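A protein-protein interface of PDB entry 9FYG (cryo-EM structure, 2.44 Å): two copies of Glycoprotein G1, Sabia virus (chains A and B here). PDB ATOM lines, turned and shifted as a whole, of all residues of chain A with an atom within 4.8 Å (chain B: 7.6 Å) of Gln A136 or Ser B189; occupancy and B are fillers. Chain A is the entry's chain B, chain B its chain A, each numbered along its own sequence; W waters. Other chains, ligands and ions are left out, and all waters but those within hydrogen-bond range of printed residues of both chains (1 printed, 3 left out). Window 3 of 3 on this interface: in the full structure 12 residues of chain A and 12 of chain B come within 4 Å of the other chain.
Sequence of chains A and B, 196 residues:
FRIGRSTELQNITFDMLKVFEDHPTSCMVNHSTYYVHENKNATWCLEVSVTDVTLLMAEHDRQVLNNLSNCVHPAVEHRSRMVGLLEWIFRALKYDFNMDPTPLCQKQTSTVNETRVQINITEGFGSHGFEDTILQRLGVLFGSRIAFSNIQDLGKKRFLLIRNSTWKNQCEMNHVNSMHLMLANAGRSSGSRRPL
Ser B189 touches Asp A132. CG2 of Thr A133 touches O of Gly B187, at 3.6 Å. CA of Arg B188 touches OG1 of Thr A133, 3.7 Å away. CB of Ser B189 touches OE1 of Gln A136 (3.9 Å).
Of the 11 printed residues of chain A, 4 touch a printed residue of chain B. Among the printed residues, 6 pairs touch across the chains.
Water W1 bridges O of Gly B187 and O of Thr A133.
No position is printed for both chains.
The backbone carbonyl oxygen of Asp A132 lies close to the side-chain amide nitrogen of Gln A136, at 3.4 Å. O of Gly A129 lies within hydrogen-bond range of OG1 of Thr A133.
N of Ser B189 lies within hydrogen-bond range of OG1 of Thr A133 (2.9 Å). The side-chain hydroxyl of Ser B189 is in hydrogen-bond range of the backbone carbonyl oxygen of Gly A129, 2.9 Å away.
Printed residues of chain B within 4 Å of Gly A129: Ser B189. Printed residues of chain B within 4 Å of Asp A132: Ser B189 (3.5 Å). Of the printed residues of chain B, Thr A133 touches Gly B187 (3.6 Å), Arg B188 (3.7 Å) and Ser B189 (2.9 Å). Of the printed residues of chain B, Gln A136 touches Ser B189. Gly A139 touches none of the printed residues of chain B. Printed residues of chain A within 4 Å of Arg B188: Thr A133 (3.7 Å). Of chain A, only Gly A129, Asp A132, Thr A133 and Gln A136 come within 4 Å of Ser B189. The nearest printed residue of chain A that does not touch Ser B189 is Ile A134 (6.5 Å).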
ATOM      1  N   GLY A 129      -1.375   4.180  25.529  1.00  0.00           N
ATOM      2  CA  GLY A 129      -1.033   5.104  24.468  1.00  0.00           C
ATOM      3  C   GLY A 129      -0.666   4.478  23.141  1.00  0.00           C
ATOM      4  O   GLY A 129      -0.347   5.214  22.201  1.00  0.00           O
ATOM      5  N   ASP A 132      -3.310   5.488  20.534  1.00  0.00           N
ATOM      6  CA  ASP A 132      -3.113   6.890  20.183  1.00  0.00           C
ATOM      7  C   ASP A 132      -1.880   7.063  19.311  1.00  0.00           C
ATOM      8  O   ASP A 132      -1.884   7.864  18.371  1.00  0.00           O
ATOM      9  CB  ASP A 132      -3.000   7.742  21.446  1.00  0.00           C
ATOM     10  CG  ASP A 132      -4.244   7.679  22.304  1.00  0.00           C
ATOM     11  OD1 ASP A 132      -5.341   7.977  21.788  1.00  0.00           O
ATOM     12  OD2 ASP A 132      -4.126   7.327  23.496  1.00  0.00           O
ATOM     13  N   THR A 133      -0.817   6.312  19.605  1.00  0.00           N
ATOM     14  CA  THR A 133       0.373   6.340  18.762  1.00  0.00           C
ATOM     15  C   THR A 133       0.038   5.927  17.335  1.00  0.00           C
ATOM     16  O   THR A 133       0.441   6.590  16.373  1.00  0.00           O
ATOM     17  CB  THR A 133       1.451   5.425  19.348  1.00  0.00           C
ATOM     18  OG1 THR A 133       1.841   5.904  20.639  1.00  0.00           O
ATOM     19  CG2 THR A 133       2.668   5.375  18.441  1.00  0.00           C
ATOM     20  N   ILE A 134      -0.724   4.842  17.181  1.00  0.00           N
ATOM     21  CA  ILE A 134      -1.071   4.358  15.848  1.00  0.00           C
ATOM     22  C   ILE A 134      -1.951   5.366  15.111  1.00  0.00           C
ATOM     23  O   ILE A 134      -1.734   5.645  13.926  1.00  0.00           O
ATOM     24  CB  ILE A 134      -1.739   2.974  15.943  1.00  0.00           C
ATOM     25  CG1 ILE A 134      -0.689   1.905  16.245  1.00  0.00           C
ATOM     26  CG2 ILE A 134      -2.485   2.641  14.659  1.00  0.00           C
ATOM     27  CD1 ILE A 134       0.426   1.833  15.218  1.00  0.00           C
ATOM     28  N   LEU A 135      -2.954   5.926  15.790  1.00  0.00           N
ATOM     29  CA  LEU A 135      -3.851   6.873  15.130  1.00  0.00           C
ATOM     30  C   LEU A 135      -3.123   8.155  14.740  1.00  0.00           C
ATOM     31  O   LEU A 135      -3.359   8.709  13.660  1.00  0.00           O
ATOM     32  CB  LEU A 135      -5.045   7.179  16.030  1.00  0.00           C
ATOM     33  CG  LEU A 135      -5.945   5.997  16.387  1.00  0.00           C
ATOM     34  CD1 LEU A 135      -7.108   6.457  17.242  1.00  0.00           C
ATOM     35  CD2 LEU A 135      -6.438   5.287  15.137  1.00  0.00           C
ATOM     36  N   GLN A 136      -2.228   8.640  15.601  1.00  0.00           N
ATOM     37  CA  GLN A 136      -1.450   9.823  15.260  1.00  0.00           C
ATOM     38  C   GLN A 136      -0.464   9.542  14.135  1.00  0.00           C
ATOM     39  O   GLN A 136      -0.208  10.419  13.303  1.00  0.00           O
ATOM     40  CB  GLN A 136      -0.735  10.341  16.504  1.00  0.00           C
ATOM     41  CG  GLN A 136      -1.660  11.068  17.463  1.00  0.00           C
ATOM     42  CD  GLN A 136      -1.128  11.106  18.875  1.00  0.00           C
ATOM     43  OE1 GLN A 136       0.070  11.266  19.096  1.00  0.00           O
ATOM     44  NE2 GLN A 136      -2.021  10.962  19.845  1.00  0.00           N
ATOM     45  N   ARG A 137       0.089   8.329  14.080  1.00  0.00           N
ATOM     46  CA  ARG A 137       0.923   7.951  12.947  1.00  0.00           C
ATOM     47  C   ARG A 137       0.112   7.912  11.658  1.00  0.00           C
ATOM     48  O   ARG A 137       0.604   8.306  10.597  1.00  0.00           O
ATOM     49  CB  ARG A 137       1.587   6.601  13.214  1.00  0.00           C
ATOM     50  CG  ARG A 137       2.718   6.274  12.265  1.00  0.00           C
ATOM     51  CD  ARG A 137       3.880   7.237  12.431  1.00  0.00           C
ATOM     52  NE  ARG A 137       4.667   7.335  11.209  1.00  0.00           N
ATOM     53  CZ  ARG A 137       5.506   8.322  10.930  1.00  0.00           C
ATOM     54  NH1 ARG A 137       5.706   9.321  11.776  1.00  0.00           N
ATOM     55  NH2 ARG A 137       6.163   8.307   9.775  1.00  0.00           N
ATOM     56  N   LEU A 138      -1.130   7.432  11.732  1.00  0.00           N
ATOM     57  CA  LEU A 138      -2.017   7.477  10.574  1.00  0.00           C
ATOM     58  C   LEU A 138      -2.268   8.912  10.134  1.00  0.00           C
ATOM     59  O   LEU A 138      -2.307   9.206   8.933  1.00  0.00           O
ATOM     60  CB  LEU A 138      -3.342   6.788  10.897  1.00  0.00           C
ATOM     61  CG  LEU A 138      -3.325   5.278  11.121  1.00  0.00           C
ATOM     62  CD1 LEU A 138      -4.613   4.839  11.787  1.00  0.00           C
ATOM     63  CD2 LEU A 138      -3.121   4.546   9.815  1.00  0.00           C
ATOM     64  N   GLY A 139      -2.459   9.815  11.095  1.00  0.00           N
ATOM     65  CA  GLY A 139      -2.622  11.219  10.755  1.00  0.00           C
ATOM     66  C   GLY A 139      -1.391  11.812  10.098  1.00  0.00           C
ATOM     67  O   GLY A 139      -1.495  12.625   9.177  1.00  0.00           O
ATOM     68  N   VAL A 140      -0.207  11.425  10.570  1.00  0.00           N
ATOM     69  CA  VAL A 140       1.028  11.905   9.959  1.00  0.00           C
ATOM     70  C   VAL A 140       1.180  11.349   8.545  1.00  0.00           C
ATOM     71  O   VAL A 140       1.620  12.055   7.629  1.00  0.00           O
ATOM     72  CB  VAL A 140       2.233  11.546  10.851  1.00  0.00           C
ATOM     73  CG1 VAL A 140       3.538  11.680  10.082  1.00  0.00           C
ATOM     74  CG2 VAL A 140       2.252  12.422  12.091  1.00  0.00           C
ATOM     75  N   ALA A 147      -7.329  10.567  15.042  1.00  0.00           N
ATOM     76  CA  ALA A 147      -6.799  10.654  16.397  1.00  0.00           C
ATOM     77  C   ALA A 147      -7.421  11.810  17.171  1.00  0.00           C
ATOM     78  O   ALA A 147      -7.479  11.768  18.405  1.00  0.00           O
ATOM     79  CB  ALA A 147      -5.280  10.803  16.362  1.00  0.00           C
ATOM     80  N   HIS B  23       4.544  14.586  30.793  1.00  0.00           N
ATOM     81  CA  HIS B  23       5.375  13.678  30.027  1.00  0.00           C
ATOM     82  C   HIS B  23       6.313  12.900  30.936  1.00  0.00           C
ATOM     83  O   HIS B  23       6.599  13.325  32.061  1.00  0.00           O
ATOM     84  CB  HIS B  23       6.186  14.454  28.979  1.00  0.00           C
ATOM     85  CG  HIS B  23       5.339  15.194  27.994  1.00  0.00           C
ATOM     86  ND1 HIS B  23       4.619  14.559  27.006  1.00  0.00           N
ATOM     87  CD2 HIS B  23       5.089  16.517  27.849  1.00  0.00           C
ATOM     88  CE1 HIS B  23       3.966  15.458  26.293  1.00  0.00           C
ATOM     89  NE2 HIS B  23       4.233  16.654  26.784  1.00  0.00           N
ATOM     90  N   PRO B  24       6.791  11.736  30.495  1.00  0.00           N
ATOM     91  CA  PRO B  24       7.760  10.989  31.305  1.00  0.00           C
ATOM     92  C   PRO B  24       9.011  11.809  31.573  1.00  0.00           C
ATOM     93  O   PRO B  24       9.515  12.519  30.702  1.00  0.00           O
ATOM     94  CB  PRO B  24       8.070   9.758  30.445  1.00  0.00           C
ATOM     95  CG  PRO B  24       6.901   9.612  29.550  1.00  0.00           C
ATOM     96  CD  PRO B  24       6.373  10.985  29.297  1.00  0.00           C
ATOM     97  N   TRP B  88       9.167   2.749  26.991  1.00  0.00           N
ATOM     98  CA  TRP B  88       9.834   4.044  26.866  1.00  0.00           C
ATOM     99  C   TRP B  88      11.284   3.956  27.327  1.00  0.00           C
ATOM    100  O   TRP B  88      12.188   4.486  26.671  1.00  0.00           O
ATOM    101  CB  TRP B  88       9.061   5.095  27.672  1.00  0.00           C
ATOM    102  CG  TRP B  88       7.734   5.503  27.066  1.00  0.00           C
ATOM    103  CD1 TRP B  88       6.559   4.842  27.186  1.00  0.00           C
ATOM    104  CD2 TRP B  88       7.422   6.732  26.400  1.00  0.00           C
ATOM    105  NE1 TRP B  88       5.552   5.515  26.555  1.00  0.00           N
ATOM    106  CE2 TRP B  88       6.054   6.692  26.074  1.00  0.00           C
ATOM    107  CE3 TRP B  88       8.165   7.851  26.030  1.00  0.00           C
ATOM    108  CZ2 TRP B  88       5.418   7.719  25.391  1.00  0.00           C
ATOM    109  CZ3 TRP B  88       7.530   8.868  25.341  1.00  0.00           C
ATOM    110  CH2 TRP B  88       6.173   8.796  25.030  1.00  0.00           C
ATOM    111  N   ARG B  91      13.337   1.854  24.768  1.00  0.00           N
ATOM    112  CA  ARG B  91      13.670   2.670  23.605  1.00  0.00           C
ATOM    113  C   ARG B  91      14.737   3.703  23.944  1.00  0.00           C
ATOM    114  O   ARG B  91      15.614   3.988  23.124  1.00  0.00           O
ATOM    115  CB  ARG B  91      12.420   3.355  23.058  1.00  0.00           C
ATOM    116  CG  ARG B  91      11.445   2.421  22.384  1.00  0.00           C
ATOM    117  CD  ARG B  91      10.344   3.192  21.683  1.00  0.00           C
ATOM    118  NE  ARG B  91       9.068   2.494  21.769  1.00  0.00           N
ATOM    119  CZ  ARG B  91       8.129   2.760  22.664  1.00  0.00           C
ATOM    120  NH1 ARG B  91       8.276   3.726  23.556  1.00  0.00           N
ATOM    121  NH2 ARG B  91       7.011   2.040  22.666  1.00  0.00           N
ATOM    122  N   ASN B 185      12.130   8.663  22.142  1.00  0.00           N
ATOM    123  CA  ASN B 185      10.792   8.102  21.998  1.00  0.00           C
ATOM    124  C   ASN B 185       9.929   8.974  21.097  1.00  0.00           C
ATOM    125  O   ASN B 185       8.751   9.213  21.378  1.00  0.00           O
ATOM    126  CB  ASN B 185      10.126   7.936  23.361  1.00  0.00           C
ATOM    127  CG  ASN B 185      10.598   6.704  24.101  1.00  0.00           C
ATOM    128  OD1 ASN B 185      10.140   5.597  23.839  1.00  0.00           O
ATOM    129  ND2 ASN B 185      11.521   6.893  25.033  1.00  0.00           N
ATOM    130  N   ALA B 186      10.504   9.468  20.005  1.00  0.00           N
ATOM    131  CA  ALA B 186       9.776  10.353  19.105  1.00  0.00           C
ATOM    132  C   ALA B 186       8.643   9.605  18.414  1.00  0.00           C
ATOM    133  O   ALA B 186       8.838   8.508  17.883  1.00  0.00           O
ATOM    134  CB  ALA B 186      10.729  10.948  18.071  1.00  0.00           C
ATOM    135  N   GLY B 187       7.454  10.208  18.415  1.00  0.00           N
ATOM    136  CA  GLY B 187       6.288   9.623  17.801  1.00  0.00           C
ATOM    137  C   GLY B 187       5.401   8.828  18.736  1.00  0.00           C
ATOM    138  O   GLY B 187       4.243   8.564  18.390  1.00  0.00           O
ATOM    139  N   ARG B 188       5.899   8.444  19.907  1.00  0.00           N
ATOM    140  CA  ARG B 188       5.102   7.697  20.870  1.00  0.00           C
ATOM    141  C   ARG B 188       4.243   8.665  21.675  1.00  0.00           C
ATOM    142  O   ARG B 188       4.760   9.621  22.262  1.00  0.00           O
ATOM    143  CB  ARG B 188       6.006   6.875  21.785  1.00  0.00           C
ATOM    144  CG  ARG B 188       6.699   5.722  21.085  1.00  0.00           C
ATOM    145  CD  ARG B 188       5.692   4.674  20.649  1.00  0.00           C
ATOM    146  NE  ARG B 188       6.229   3.776  19.633  1.00  0.00           N
ATOM    147  CZ  ARG B 188       5.669   2.627  19.282  1.00  0.00           C
ATOM    148  NH1 ARG B 188       4.553   2.200  19.848  1.00  0.00           N
ATOM    149  NH2 ARG B 188       6.246   1.885  18.339  1.00  0.00           N
ATOM    150  N   SER B 189       2.937   8.415  21.702  1.00  0.00           N
ATOM    151  CA  SER B 189       2.006   9.340  22.333  1.00  0.00           C
ATOM    152  C   SER B 189       2.269   9.474  23.829  1.00  0.00           C
ATOM    153  O   SER B 189       2.549   8.493  24.524  1.00  0.00           O
ATOM    154  CB  SER B 189       0.566   8.883  22.089  1.00  0.00           C
ATOM    155  OG  SER B 189       0.145   7.956  23.071  1.00  0.00           O
ATOM    156  N   SER B 190       2.174  10.709  24.320  1.00  0.00           N
ATOM    157  CA  SER B 190       2.291  11.006  25.739  1.00  0.00           C
ATOM    158  C   SER B 190       1.557  12.308  26.024  1.00  0.00           C
ATOM    159  O   SER B 190       1.174  13.043  25.111  1.00  0.00           O
ATOM    160  CB  SER B 190       3.755  11.103  26.183  1.00  0.00           C
ATOM    161  OG  SER B 190       4.403  12.210  25.583  1.00  0.00           O
ATOM    162  N   GLY B 191       1.358  12.584  27.308  1.00  0.00           N
ATOM    163  CA  GLY B 191       0.742  13.830  27.719  1.00  0.00           C
ATOM    164  C   GLY B 191      -0.757  13.732  27.902  1.00  0.00           C
ATOM    165  O   GLY B 191      -1.494  13.499  26.939  1.00  0.00           O
HETATM  166  O   HOH W   1       2.966   8.300  16.099  1.00  0.00           O
